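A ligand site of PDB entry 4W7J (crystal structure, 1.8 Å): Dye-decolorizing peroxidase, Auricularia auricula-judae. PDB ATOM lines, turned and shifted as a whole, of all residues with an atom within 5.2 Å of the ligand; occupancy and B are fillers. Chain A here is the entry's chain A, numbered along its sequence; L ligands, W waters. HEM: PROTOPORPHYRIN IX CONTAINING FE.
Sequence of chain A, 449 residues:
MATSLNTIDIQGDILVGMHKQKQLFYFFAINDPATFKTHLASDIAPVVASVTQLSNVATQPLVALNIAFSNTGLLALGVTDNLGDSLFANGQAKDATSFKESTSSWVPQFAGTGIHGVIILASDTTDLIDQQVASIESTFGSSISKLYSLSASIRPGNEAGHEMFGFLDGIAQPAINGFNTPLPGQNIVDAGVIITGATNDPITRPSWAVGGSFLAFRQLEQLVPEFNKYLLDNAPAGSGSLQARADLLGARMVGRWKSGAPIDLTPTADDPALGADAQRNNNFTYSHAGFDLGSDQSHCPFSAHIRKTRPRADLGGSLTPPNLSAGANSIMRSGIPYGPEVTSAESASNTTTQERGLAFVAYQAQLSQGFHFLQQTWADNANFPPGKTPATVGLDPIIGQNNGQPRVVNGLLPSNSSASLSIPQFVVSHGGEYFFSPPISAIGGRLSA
O1A of the ligand is in salt-bridge range of NE of Arg 256, 2.9 Å away.
O1D of the ligand lies within salt-bridge range of NH2 of Arg 312, at 3.0 Å.
An oxygen (O2A) of the ligand lies within hydrogen-bond range of the backbone NH of Ile 171 (2.9 Å).
NH2 of Arg 333 lies within salt-bridge range of O2A of the ligand (2.6 Å).
FE of the ligand is bound by NE2 of His 305, at 2.3 Å.
An oxygen (O2A) of the ligand sits at hydrogen-bond distance from the backbone NH (N) of Ala 172 (3.0 Å).
O2A of the ligand sits at hydrogen-bond distance from N of Gly 170 (3.4 Å).
Water W5 bridges an oxygen (O1A) of the ligand (2.6 Å) and the guanidinium group of Arg 256 (2.7 Å).
Water W2 lies within hydrogen-bond range of the backbone carbonyl oxygen of Arg 310 (2.6 Å), the side-chain hydroxyl of Tyr 286 (2.7 Å), an oxygen (O1D) of the ligand (2.7 Å), the backbone carbonyl oxygen of Ile 306 (2.8 Å) and the guanidinium group of Arg 312 (3.0 Å).
Residues that only touch the ligand: Glu 163 (3.3 Å), Phe 165 (3.9 Å), Phe 167 (3.5 Å), Leu 168 (3.5 Å), Asp 169 (3.7 Å), Leu 220 (3.8 Å), Gln 222 (3.5 Å), Val 254 (3.7 Å), Ile 306 (3.6 Å), Thr 309 (3.2 Å), Arg 310 (3.4 Å), Ile 331 (3.9 Å), Leu 358 (3.8 Å), Phe 360 (3.2 Å), Phe 371 (3.4 Å), Leu 374 (3.9 Å), Gln 375 (3.7 Å), Ile 398 (3.8 Å), Ile 399 (3.4 Å) and Val 427 (3.7 Å).
27 residues have an atom within 4 Å of the ligand: Glu 163, Phe 165, Phe 167, Leu 168, Asp 169, Gly 170, Ile 171, Ala 172, Leu 220, Gln 222, Val 254, Arg 256, His 305, Ile 306, Thr 309, Arg 310, Arg 312, Ile 331, Arg 333, Leu 358, Phe 360, Phe 371, Leu 374, Gln 375, Ile 398, Ile 399 and Val 427.
Along chain A the residues within 4 Å of the ligand span positions 163 to 427.
The nearest printed residue that does not touch the ligand is Asn 282 (4.9 Å).
N of Ile 306 is in hydrogen-bond range of O of Val 254 (3.0 Å).
The backbone NH (N) of His 305 lies within hydrogen-bond range of the backbone carbonyl oxygen (O) of Val 254, at 3.3 Å.
NH2 of Arg 333 lies within hydrogen-bond range of O of Ala 172 (2.9 Å).
O of Ile 306 lies within hydrogen-bond range of OG1 of Thr 309.
OE2 of Glu 163 lies within hydrogen-bond range of NE2 of Gln 222, 2.7 Å away.
OE1 of Glu 163 lies within hydrogen-bond range of N of Phe 167, 2.8 Å away.
The side-chain amide oxygen (OE1) of Gln 222 lies within hydrogen-bond range of the backbone NH (N) of Leu 358.
NE2 of Gln 222 lies close to N of Phe 165, 3.5 Å away.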
ATOM      1  N   GLU A 163       4.307  -9.881  23.317  1.00  0.00           N
ATOM      2  CA  GLU A 163       4.578  -8.853  22.322  1.00  0.00           C
ATOM      3  C   GLU A 163       6.093  -8.870  21.996  1.00  0.00           C
ATOM      4  O   GLU A 163       6.830  -9.735  22.496  1.00  0.00           O
ATOM      5  CB  GLU A 163       4.071  -7.485  22.800  1.00  0.00           C
ATOM      6  CG  GLU A 163       4.464  -7.090  24.220  1.00  0.00           C
ATOM      7  CD  GLU A 163       5.920  -6.767  24.317  1.00  0.00           C
ATOM      8  OE1 GLU A 163       6.624  -7.362  25.181  1.00  0.00           O
ATOM      9  OE2 GLU A 163       6.371  -5.924  23.505  1.00  0.00           O
ATOM     10  N   PHE A 165       8.782  -7.092  22.714  1.00  0.00           N
ATOM     11  CA  PHE A 165       9.795  -6.999  23.777  1.00  0.00           C
ATOM     12  C   PHE A 165       9.884  -8.307  24.575  1.00  0.00           C
ATOM     13  O   PHE A 165      10.791  -8.504  25.394  1.00  0.00           O
ATOM     14  CB  PHE A 165       9.509  -5.825  24.736  1.00  0.00           C
ATOM     15  CG  PHE A 165       9.724  -4.455  24.127  1.00  0.00           C
ATOM     16  CD1 PHE A 165      10.759  -4.223  23.235  1.00  0.00           C
ATOM     17  CD2 PHE A 165       8.896  -3.403  24.482  1.00  0.00           C
ATOM     18  CE1 PHE A 165      10.947  -2.952  22.676  1.00  0.00           C
ATOM     19  CE2 PHE A 165       9.073  -2.125  23.941  1.00  0.00           C
ATOM     20  CZ  PHE A 165      10.109  -1.907  23.038  1.00  0.00           C
ATOM     21  N   PHE A 167       7.152  -9.772  26.408  1.00  0.00           N
ATOM     22  CA  PHE A 167       6.286  -9.834  27.571  1.00  0.00           C
ATOM     23  C   PHE A 167       4.910 -10.392  27.221  1.00  0.00           C
ATOM     24  O   PHE A 167       4.284  -9.959  26.256  1.00  0.00           O
ATOM     25  CB  PHE A 167       6.124  -8.459  28.216  1.00  0.00           C
ATOM     26  CG  PHE A 167       7.396  -7.908  28.829  1.00  0.00           C
ATOM     27  CD1 PHE A 167       8.381  -7.323  28.041  1.00  0.00           C
ATOM     28  CD2 PHE A 167       7.598  -7.962  30.206  1.00  0.00           C
ATOM     29  CE1 PHE A 167       9.548  -6.813  28.607  1.00  0.00           C
ATOM     30  CE2 PHE A 167       8.773  -7.455  30.767  1.00  0.00           C
ATOM     31  CZ  PHE A 167       9.742  -6.877  29.978  1.00  0.00           C
ATOM     32  N   LEU A 168       4.443 -11.361  28.017  1.00  0.00           N
ATOM     33  CA  LEU A 168       3.111 -11.914  27.829  1.00  0.00           C
ATOM     34  C   LEU A 168       2.081 -10.790  27.891  1.00  0.00           C
ATOM     35  O   LEU A 168       2.118  -9.942  28.792  1.00  0.00           O
ATOM     36  CB  LEU A 168       2.815 -12.991  28.869  1.00  0.00           C
ATOM     37  CG  LEU A 168       1.438 -13.655  28.708  1.00  0.00           C
ATOM     38  CD1 LEU A 168       1.311 -14.416  27.391  1.00  0.00           C
ATOM     39  CD2 LEU A 168       1.109 -14.563  29.877  1.00  0.00           C
ATOM     40  N   ASP A 169       1.173 -10.781  26.919  1.00  0.00           N
ATOM     41  CA  ASP A 169       0.273  -9.657  26.702  1.00  0.00           C
ATOM     42  C   ASP A 169      -1.167 -10.165  26.631  1.00  0.00           C
ATOM     43  O   ASP A 169      -1.394 -11.343  26.354  1.00  0.00           O
ATOM     44  CB  ASP A 169       0.668  -8.935  25.406  1.00  0.00           C
ATOM     45  CG  ASP A 169      -0.065  -7.615  25.195  1.00  0.00           C
ATOM     46  OD1 ASP A 169      -0.492  -6.990  26.182  1.00  0.00           O
ATOM     47  OD2 ASP A 169      -0.183  -7.191  24.024  1.00  0.00           O
ATOM     48  N   GLY A 170      -2.147  -9.301  26.886  1.00  0.00           N
ATOM     49  CA  GLY A 170      -3.544  -9.708  26.791  1.00  0.00           C
ATOM     50  C   GLY A 170      -4.047 -10.350  28.069  1.00  0.00           C
ATOM     51  O   GLY A 170      -5.039 -11.077  28.077  1.00  0.00           O
ATOM     52  N   ILE A 171      -3.360 -10.080  29.168  1.00  0.00           N
ATOM     53  CA  ILE A 171      -3.771 -10.582  30.458  1.00  0.00           C
ATOM     54  C   ILE A 171      -4.893  -9.742  31.062  1.00  0.00           C
ATOM     55  O   ILE A 171      -5.902 -10.274  31.537  1.00  0.00           O
ATOM     56  CB  ILE A 171      -2.579 -10.582  31.444  1.00  0.00           C
ATOM     57  CG1 ILE A 171      -1.465 -11.503  30.948  1.00  0.00           C
ATOM     58  CG2 ILE A 171      -3.038 -10.984  32.819  1.00  0.00           C
ATOM     59  CD1 ILE A 171      -0.198 -11.497  31.836  1.00  0.00           C
ATOM     60  N   ALA A 172      -4.722  -8.430  31.029  1.00  0.00           N
ATOM     61  CA  ALA A 172      -5.581  -7.528  31.778  1.00  0.00           C
ATOM     62  C   ALA A 172      -6.593  -6.808  30.870  1.00  0.00           C
ATOM     63  O   ALA A 172      -6.204  -6.112  29.942  1.00  0.00           O
ATOM     64  CB  ALA A 172      -4.729  -6.501  32.528  1.00  0.00           C
ATOM     65  N   GLN A 173      -7.873  -7.017  31.140  1.00  0.00           N
ATOM     66  CA  GLN A 173      -8.938  -6.262  30.495  1.00  0.00           C
ATOM     67  C   GLN A 173     -10.000  -5.857  31.513  1.00  0.00           C
ATOM     68  O   GLN A 173     -10.160  -6.496  32.537  1.00  0.00           O
ATOM     69  CB  GLN A 173      -9.599  -7.091  29.383  1.00  0.00           C
ATOM     70  CG  GLN A 173      -8.624  -7.777  28.432  1.00  0.00           C
ATOM     71  CD  GLN A 173      -8.157  -6.880  27.292  1.00  0.00           C
ATOM     72  OE1 GLN A 173      -8.388  -5.670  27.283  1.00  0.00           O
ATOM     73  NE2 GLN A 173      -7.508  -7.486  26.312  1.00  0.00           N
ATOM     74  N   LEU A 220       2.836   0.827  16.222  1.00  0.00           N
ATOM     75  CA  LEU A 220       3.926   1.166  17.143  1.00  0.00           C
ATOM     76  C   LEU A 220       5.184   0.321  16.943  1.00  0.00           C
ATOM     77  O   LEU A 220       5.252  -0.804  17.404  1.00  0.00           O
ATOM     78  CB  LEU A 220       3.432   1.014  18.583  1.00  0.00           C
ATOM     79  CG  LEU A 220       2.228   1.910  18.876  1.00  0.00           C
ATOM     80  CD1 LEU A 220       1.704   1.676  20.294  1.00  0.00           C
ATOM     81  CD2 LEU A 220       2.588   3.387  18.668  1.00  0.00           C
ATOM     82  N   GLN A 222       8.747  -1.170  17.647  1.00  0.00           N
ATOM     83  CA  GLN A 222       9.532  -1.421  18.841  1.00  0.00           C
ATOM     84  C   GLN A 222      10.974  -1.710  18.487  1.00  0.00           C
ATOM     85  O   GLN A 222      11.268  -2.542  17.630  1.00  0.00           O
ATOM     86  CB  GLN A 222       8.952  -2.594  19.644  1.00  0.00           C
ATOM     87  CG  GLN A 222       7.558  -2.322  20.159  1.00  0.00           C
ATOM     88  CD  GLN A 222       6.862  -3.570  20.647  1.00  0.00           C
ATOM     89  OE1 GLN A 222       5.939  -4.070  20.012  1.00  0.00           O
ATOM     90  NE2 GLN A 222       7.302  -4.072  21.801  1.00  0.00           N
ATOM     91  N   VAL A 254       7.789  -2.417  32.759  1.00  0.00           N
ATOM     92  CA  VAL A 254       6.452  -2.863  32.337  1.00  0.00           C
ATOM     93  C   VAL A 254       5.456  -2.932  33.492  1.00  0.00           C
ATOM     94  O   VAL A 254       4.298  -2.510  33.356  1.00  0.00           O
ATOM     95  CB  VAL A 254       6.508  -4.253  31.669  1.00  0.00           C
ATOM     96  CG1 VAL A 254       5.098  -4.738  31.287  1.00  0.00           C
ATOM     97  CG2 VAL A 254       7.417  -4.220  30.455  1.00  0.00           C
ATOM     98  N   ARG A 256       5.064  -5.942  34.754  1.00  0.00           N
ATOM     99  CA  ARG A 256       4.993  -7.400  34.731  1.00  0.00           C
ATOM    100  C   ARG A 256       6.324  -7.974  34.256  1.00  0.00           C
ATOM    101  O   ARG A 256       7.030  -7.343  33.470  1.00  0.00           O
ATOM    102  CB  ARG A 256       3.879  -7.890  33.813  1.00  0.00           C
ATOM    103  CG  ARG A 256       2.476  -7.651  34.313  1.00  0.00           C
ATOM    104  CD  ARG A 256       1.437  -8.289  33.357  1.00  0.00           C
ATOM    105  NE  ARG A 256       0.099  -7.876  33.752  1.00  0.00           N
ATOM    106  CZ  ARG A 256      -0.609  -8.449  34.715  1.00  0.00           C
ATOM    107  NH1 ARG A 256      -0.129  -9.510  35.378  1.00  0.00           N
ATOM    108  NH2 ARG A 256      -1.799  -7.971  35.018  1.00  0.00           N
ATOM    109  N   ASN A 282      -3.725 -11.088  38.232  1.00  0.00           N
ATOM    110  CA  ASN A 282      -4.215  -9.721  38.276  1.00  0.00           C
ATOM    111  C   ASN A 282      -4.679  -9.316  39.666  1.00  0.00           C
ATOM    112  O   ASN A 282      -5.263  -8.254  39.857  1.00  0.00           O
ATOM    113  CB  ASN A 282      -5.362  -9.520  37.293  1.00  0.00           C
ATOM    114  CG  ASN A 282      -5.254  -8.205  36.567  1.00  0.00           C
ATOM    115  OD1 ASN A 282      -4.225  -7.540  36.648  1.00  0.00           O
ATOM    116  ND2 ASN A 282      -6.305  -7.832  35.855  1.00  0.00           N
ATOM    117  N   TYR A 286      -1.604  -2.604  44.131  1.00  0.00           N
ATOM    118  CA  TYR A 286      -0.375  -1.839  44.432  1.00  0.00           C
ATOM    119  C   TYR A 286      -0.285  -1.464  45.911  1.00  0.00           C
ATOM    120  O   TYR A 286       0.735  -0.940  46.358  1.00  0.00           O
ATOM    121  CB  TYR A 286      -0.228  -0.573  43.563  1.00  0.00           C
ATOM    122  CG  TYR A 286      -0.154  -0.888  42.077  1.00  0.00           C
ATOM    123  CD1 TYR A 286       0.844  -1.712  41.580  1.00  0.00           C
ATOM    124  CD2 TYR A 286      -1.093  -0.387  41.185  1.00  0.00           C
ATOM    125  CE1 TYR A 286       0.916  -2.017  40.240  1.00  0.00           C
ATOM    126  CE2 TYR A 286      -1.032  -0.694  39.829  1.00  0.00           C
ATOM    127  CZ  TYR A 286      -0.025  -1.513  39.361  1.00  0.00           C
ATOM    128  OH  TYR A 286       0.044  -1.815  38.035  1.00  0.00           O
ATOM    129  N   HIS A 305       4.672   0.769  33.365  1.00  0.00           N
ATOM    130  CA  HIS A 305       3.673   0.925  32.309  1.00  0.00           C
ATOM    131  C   HIS A 305       2.248   0.619  32.769  1.00  0.00           C
ATOM    132  O   HIS A 305       1.364   1.452  32.575  1.00  0.00           O
ATOM    133  CB  HIS A 305       4.033   0.042  31.122  1.00  0.00           C
ATOM    134  CG  HIS A 305       3.034   0.114  30.013  1.00  0.00           C
ATOM    135  ND1 HIS A 305       2.607   1.302  29.462  1.00  0.00           N
ATOM    136  CD2 HIS A 305       2.374  -0.872  29.348  1.00  0.00           C
ATOM    137  CE1 HIS A 305       1.718   1.053  28.520  1.00  0.00           C
ATOM    138  NE2 HIS A 305       1.560  -0.255  28.436  1.00  0.00           N
ATOM    139  N   ILE A 306       2.010  -0.541  33.366  1.00  0.00           N
ATOM    140  CA  ILE A 306       0.621  -0.892  33.695  1.00  0.00           C
ATOM    141  C   ILE A 306       0.097  -0.082  34.878  1.00  0.00           C
ATOM    142  O   ILE A 306      -1.110   0.124  35.007  1.00  0.00           O
ATOM    143  CB  ILE A 306       0.435  -2.408  33.983  1.00  0.00           C
ATOM    144  CG1 ILE A 306       1.165  -2.838  35.262  1.00  0.00           C
ATOM    145  CG2 ILE A 306       0.885  -3.250  32.780  1.00  0.00           C
ATOM    146  CD1 ILE A 306       0.636  -4.176  35.826  1.00  0.00           C
ATOM    147  N   THR A 309      -1.140   3.057  33.323  1.00  0.00           N
ATOM    148  CA  THR A 309      -2.312   2.945  32.464  1.00  0.00           C
ATOM    149  C   THR A 309      -3.526   2.391  33.187  1.00  0.00           C
ATOM    150  O   THR A 309      -4.662   2.610  32.750  1.00  0.00           O
ATOM    151  CB  THR A 309      -2.032   2.077  31.221  1.00  0.00           C
ATOM    152  OG1 THR A 309      -1.666   0.744  31.618  1.00  0.00           O
ATOM    153  CG2 THR A 309      -0.919   2.699  30.380  1.00  0.00           C
ATOM    154  N   ARG A 310      -3.290   1.679  34.288  1.00  0.00           N
ATOM    155  CA  ARG A 310      -4.346   1.363  35.249  1.00  0.00           C
ATOM    156  C   ARG A 310      -3.831   1.558  36.674  1.00  0.00           C
ATOM    157  O   ARG A 310      -3.254   0.639  37.261  1.00  0.00           O
ATOM    158  CB  ARG A 310      -4.875  -0.057  35.071  1.00  0.00           C
ATOM    159  CG  ARG A 310      -6.128  -0.296  35.916  1.00  0.00           C
ATOM    160  CD  ARG A 310      -6.505  -1.762  36.111  1.00  0.00           C
ATOM    161  NE  ARG A 310      -7.481  -1.892  37.196  1.00  0.00           N
ATOM    162  CZ  ARG A 310      -7.825  -3.044  37.779  1.00  0.00           C
ATOM    163  NH1 ARG A 310      -7.299  -4.193  37.369  1.00  0.00           N
ATOM    164  NH2 ARG A 310      -8.702  -3.045  38.777  1.00  0.00           N
ATOM    165  N   ARG A 312      -5.102   1.735  39.635  1.00  0.00           N
ATOM    166  CA  ARG A 312      -5.675   0.992  40.762  1.00  0.00           C
ATOM    167  C   ARG A 312      -5.706   1.847  42.033  1.00  0.00           C
ATOM    168  O   ARG A 312      -6.310   2.925  42.031  1.00  0.00           O
ATOM    169  CB  ARG A 312      -4.918  -0.323  40.970  1.00  0.00           C
ATOM    170  CG  ARG A 312      -4.840  -1.141  39.676  1.00  0.00           C
ATOM    171  CD  ARG A 312      -4.396  -2.588  39.850  1.00  0.00           C
ATOM    172  NE  ARG A 312      -4.133  -3.215  38.551  1.00  0.00           N
ATOM    173  CZ  ARG A 312      -4.257  -4.515  38.286  1.00  0.00           C
ATOM    174  NH1 ARG A 312      -4.651  -5.364  39.229  1.00  0.00           N
ATOM    175  NH2 ARG A 312      -3.990  -4.962  37.055  1.00  0.00           N
ATOM    176  N   ILE A 331      -9.892   0.566  28.882  1.00  0.00           N
ATOM    177  CA  ILE A 331      -9.909   0.271  27.456  1.00  0.00           C
ATOM    178  C   ILE A 331      -9.824  -1.229  27.235  1.00  0.00           C
ATOM    179  O   ILE A 331      -9.176  -1.935  28.012  1.00  0.00           O
ATOM    180  CB  ILE A 331      -8.742   0.953  26.707  1.00  0.00           C
ATOM    181  CG1 ILE A 331      -7.399   0.497  27.301  1.00  0.00           C
ATOM    182  CG2 ILE A 331      -8.878   2.474  26.780  1.00  0.00           C
ATOM    183  CD1 ILE A 331      -6.197   0.833  26.422  1.00  0.00           C
ATOM    184  N   ARG A 333      -8.119  -4.015  24.904  1.00  0.00           N
ATOM    185  CA  ARG A 333      -6.962  -4.053  24.035  1.00  0.00           C
ATOM    186  C   ARG A 333      -6.965  -5.328  23.216  1.00  0.00           C
ATOM    187  O   ARG A 333      -7.143  -6.418  23.756  1.00  0.00           O
ATOM    188  CB  ARG A 333      -5.653  -3.954  24.863  1.00  0.00           C
ATOM    189  CG  ARG A 333      -5.448  -2.602  25.552  1.00  0.00           C
ATOM    190  CD  ARG A 333      -4.234  -2.655  26.504  1.00  0.00           C
ATOM    191  NE  ARG A 333      -4.373  -3.764  27.441  1.00  0.00           N
ATOM    192  CZ  ARG A 333      -3.508  -4.770  27.540  1.00  0.00           C
ATOM    193  NH1 ARG A 333      -2.417  -4.782  26.786  1.00  0.00           N
ATOM    194  NH2 ARG A 333      -3.730  -5.750  28.414  1.00  0.00           N
ATOM    195  N   LEU A 358       4.121  -3.389  17.549  1.00  0.00           N
ATOM    196  CA  LEU A 358       2.790  -3.781  17.988  1.00  0.00           C
ATOM    197  C   LEU A 358       1.754  -3.081  17.110  1.00  0.00           C
ATOM    198  O   LEU A 358       1.801  -1.854  16.949  1.00  0.00           O
ATOM    199  CB  LEU A 358       2.563  -3.398  19.450  1.00  0.00           C
ATOM    200  CG  LEU A 358       1.234  -3.823  20.083  1.00  0.00           C
ATOM    201  CD1 LEU A 358       1.116  -5.348  20.192  1.00  0.00           C
ATOM    202  CD2 LEU A 358       1.076  -3.171  21.454  1.00  0.00           C
ATOM    203  N   PHE A 360      -1.246  -1.893  17.631  1.00  0.00           N
ATOM    204  CA  PHE A 360      -2.013  -1.564  18.819  1.00  0.00           C
ATOM    205  C   PHE A 360      -3.473  -1.272  18.473  1.00  0.00           C
ATOM    206  O   PHE A 360      -3.747  -0.543  17.516  1.00  0.00           O
ATOM    207  CB  PHE A 360      -1.379  -0.357  19.521  1.00  0.00           C
ATOM    208  CG  PHE A 360      -2.135   0.119  20.728  1.00  0.00           C
ATOM    209  CD1 PHE A 360      -1.913  -0.448  21.961  1.00  0.00           C
ATOM    210  CD2 PHE A 360      -3.041   1.172  20.616  1.00  0.00           C
ATOM    211  CE1 PHE A 360      -2.595   0.007  23.083  1.00  0.00           C
ATOM    212  CE2 PHE A 360      -3.732   1.635  21.719  1.00  0.00           C
ATOM    213  CZ  PHE A 360      -3.514   1.049  22.956  1.00  0.00           C
ATOM    214  N   PHE A 371      -7.923   5.684  25.271  1.00  0.00           N
ATOM    215  CA  PHE A 371      -6.558   5.768  24.737  1.00  0.00           C
ATOM    216  C   PHE A 371      -5.912   7.148  24.887  1.00  0.00           C
ATOM    217  O   PHE A 371      -4.823   7.275  25.438  1.00  0.00           O
ATOM    218  CB  PHE A 371      -6.532   5.379  23.253  1.00  0.00           C
ATOM    219  CG  PHE A 371      -5.298   5.848  22.547  1.00  0.00           C
ATOM    220  CD1 PHE A 371      -4.056   5.262  22.821  1.00  0.00           C
ATOM    221  CD2 PHE A 371      -5.358   6.899  21.640  1.00  0.00           C
ATOM    222  CE1 PHE A 371      -2.915   5.714  22.191  1.00  0.00           C
ATOM    223  CE2 PHE A 371      -4.206   7.358  21.003  1.00  0.00           C
ATOM    224  CZ  PHE A 371      -2.986   6.763  21.267  1.00  0.00           C
ATOM    225  N   LEU A 374      -5.171   7.990  28.572  1.00  0.00           N
ATOM    226  CA  LEU A 374      -4.071   7.227  29.159  1.00  0.00           C
ATOM    227  C   LEU A 374      -2.725   7.696  28.608  1.00  0.00           C
ATOM    228  O   LEU A 374      -1.758   7.825  29.350  1.00  0.00           O
ATOM    229  CB  LEU A 374      -4.223   5.715  28.904  1.00  0.00           C
ATOM    230  CG  LEU A 374      -5.522   4.993  29.238  1.00  0.00           C
ATOM    231  CD1 LEU A 374      -5.327   3.482  29.367  1.00  0.00           C
ATOM    232  CD2 LEU A 374      -6.213   5.573  30.454  1.00  0.00           C
ATOM    233  N   GLN A 375      -2.662   7.975  27.314  1.00  0.00           N
ATOM    234  CA  GLN A 375      -1.421   8.431  26.702  1.00  0.00           C
ATOM    235  C   GLN A 375      -0.990   9.818  27.225  1.00  0.00           C
ATOM    236  O   GLN A 375       0.145   9.987  27.670  1.00  0.00           O
ATOM    237  CB  GLN A 375      -1.561   8.473  25.177  1.00  0.00           C
ATOM    238  CG  GLN A 375      -0.268   8.775  24.420  1.00  0.00           C
ATOM    239  CD  GLN A 375       0.745   7.639  24.491  1.00  0.00           C
ATOM    240  OE1 GLN A 375       0.470   6.514  24.073  1.00  0.00           O
ATOM    241  NE2 GLN A 375       1.926   7.940  25.016  1.00  0.00           N
ATOM    242  N   ILE A 398       7.734   2.670  28.710  1.00  0.00           N
ATOM    243  CA  ILE A 398       7.390   1.916  27.514  1.00  0.00           C
ATOM    244  C   ILE A 398       6.765   2.828  26.453  1.00  0.00           C
ATOM    245  O   ILE A 398       7.233   2.872  25.316  1.00  0.00           O
ATOM    246  CB  ILE A 398       6.443   0.734  27.827  1.00  0.00           C
ATOM    247  CG1 ILE A 398       7.032  -0.187  28.913  1.00  0.00           C
ATOM    248  CG2 ILE A 398       6.076  -0.037  26.527  1.00  0.00           C
ATOM    249  CD1 ILE A 398       8.371  -0.862  28.561  1.00  0.00           C
ATOM    250  N   ILE A 399       5.726   3.570  26.815  1.00  0.00           N
ATOM    251  CA  ILE A 399       5.025   4.365  25.814  1.00  0.00           C
ATOM    252  C   ILE A 399       5.104   5.873  26.033  1.00  0.00           C
ATOM    253  O   ILE A 399       4.592   6.636  25.209  1.00  0.00           O
ATOM    254  CB  ILE A 399       3.516   3.975  25.745  1.00  0.00           C
ATOM    255  CG1 ILE A 399       2.793   4.358  27.032  1.00  0.00           C
ATOM    256  CG2 ILE A 399       3.352   2.509  25.447  1.00  0.00           C
ATOM    257  CD1 ILE A 399       1.286   4.181  26.934  1.00  0.00           C
ATOM    258  N   VAL A 427       9.838   2.649  21.766  1.00  0.00           N
ATOM    259  CA  VAL A 427       8.615   2.556  20.952  1.00  0.00           C
ATOM    260  C   VAL A 427       8.520   3.828  20.124  1.00  0.00           C
ATOM    261  O   VAL A 427       8.537   4.938  20.668  1.00  0.00           O
ATOM    262  CB  VAL A 427       7.357   2.365  21.822  1.00  0.00           C
ATOM    263  CG1 VAL A 427       6.078   2.384  20.940  1.00  0.00           C
ATOM    264  CG2 VAL A 427       7.421   1.051  22.565  1.00  0.00           C
HETATM  265  CHA HEM L   1      -0.713  -3.740  29.558  1.00  0.00           C
HETATM  266  CHB HEM L   1       3.017  -3.607  26.494  1.00  0.00           C
HETATM  267  CHC HEM L   1       1.117   0.209  24.211  1.00  0.00           C
HETATM  268  CHD HEM L   1      -2.254   0.525  27.675  1.00  0.00           C
HETATM  269  C1A HEM L   1       0.455  -4.058  28.908  1.00  0.00           C
HETATM  270  C2A HEM L   1       1.333  -5.185  29.188  1.00  0.00           C
HETATM  271  C3A HEM L   1       2.346  -5.138  28.338  1.00  0.00           C
HETATM  272  C4A HEM L   1       2.157  -3.988  27.485  1.00  0.00           C
HETATM  273  CMA HEM L   1       3.550  -6.099  28.231  1.00  0.00           C
HETATM  274  CAA HEM L   1       1.113  -6.241  30.296  1.00  0.00           C
HETATM  275  CBA HEM L   1       0.135  -7.297  29.788  1.00  0.00           C
HETATM  276  CGA HEM L   1      -1.229  -7.097  30.386  1.00  0.00           C
HETATM  277  O1A HEM L   1      -1.335  -6.592  31.552  1.00  0.00           O
HETATM  278  O2A HEM L   1      -2.214  -7.460  29.698  1.00  0.00           O
HETATM  279  C1B HEM L   1       2.830  -2.565  25.624  1.00  0.00           C
HETATM  280  C2B HEM L   1       3.739  -2.221  24.555  1.00  0.00           C
HETATM  281  C3B HEM L   1       3.221  -1.150  23.905  1.00  0.00           C
HETATM  282  C4B HEM L   1       1.969  -0.817  24.550  1.00  0.00           C
HETATM  283  CMB HEM L   1       5.055  -2.978  24.285  1.00  0.00           C
HETATM  284  CAB HEM L   1       3.805  -0.419  22.686  1.00  0.00           C
HETATM  285  CBB HEM L   1       4.510  -1.066  21.757  1.00  0.00           C
HETATM  286  C1C HEM L   1       0.091   0.651  24.997  1.00  0.00           C
HETATM  287  C2C HEM L   1      -0.608   1.899  24.817  1.00  0.00           C
HETATM  288  C3C HEM L   1      -1.550   1.984  25.767  1.00  0.00           C
HETATM  289  C4C HEM L   1      -1.447   0.804  26.595  1.00  0.00           C
HETATM  290  CMC HEM L   1      -0.284   2.877  23.682  1.00  0.00           C
HETATM  291  CAC HEM L   1      -2.565   3.112  26.060  1.00  0.00           C
HETATM  292  CBC HEM L   1      -2.380   4.391  25.683  1.00  0.00           C
HETATM  293  C1D HEM L   1      -2.228  -0.620  28.444  1.00  0.00           C
HETATM  294  C2D HEM L   1      -3.223  -0.999  29.417  1.00  0.00           C
HETATM  295  C3D HEM L   1      -2.745  -2.325  30.004  1.00  0.00           C
HETATM  296  C4D HEM L   1      -1.502  -2.621  29.326  1.00  0.00           C
HETATM  297  CMD HEM L   1      -4.521  -0.259  29.820  1.00  0.00           C
HETATM  298  CAD HEM L   1      -3.500  -3.123  31.089  1.00  0.00           C
HETATM  299  CBD HEM L   1      -3.160  -2.473  32.428  1.00  0.00           C
HETATM  300  CGD HEM L   1      -3.990  -3.029  33.557  1.00  0.00           C
HETATM  301  O1D HEM L   1      -3.428  -3.168  34.674  1.00  0.00           O
HETATM  302  O2D HEM L   1      -5.208  -3.314  33.369  1.00  0.00           O
HETATM  303  NA  HEM L   1       0.990  -3.354  27.857  1.00  0.00           N
HETATM  304  NB  HEM L   1       1.752  -1.687  25.605  1.00  0.00           N
HETATM  305  NC  HEM L   1      -0.432  -0.003  26.097  1.00  0.00           N
HETATM  306  ND  HEM L   1      -1.235  -1.594  28.419  1.00  0.00           N
HETATM  307 FE   HEM L   1       0.336  -1.614  27.090  1.00  0.00          FE
HETATM  308  O   HOH W   1       0.994   5.408  21.779  1.00  0.00           O
HETATM  309  O   HOH W   2      -2.287  -1.762  36.710  1.00  0.00           O
HETATM  310  O   HOH W   3      -7.008  -2.871  31.478  1.00  0.00           O
HETATM  311  O   HOH W   4      -0.928  -2.900  25.260  1.00  0.00           O
HETATM  312  O   HOH W   5      -1.888  -5.513  33.891  1.00  0.00           O
HETATM  313  O   HOH W   6      -6.537  -4.968  34.890  1.00  0.00           O
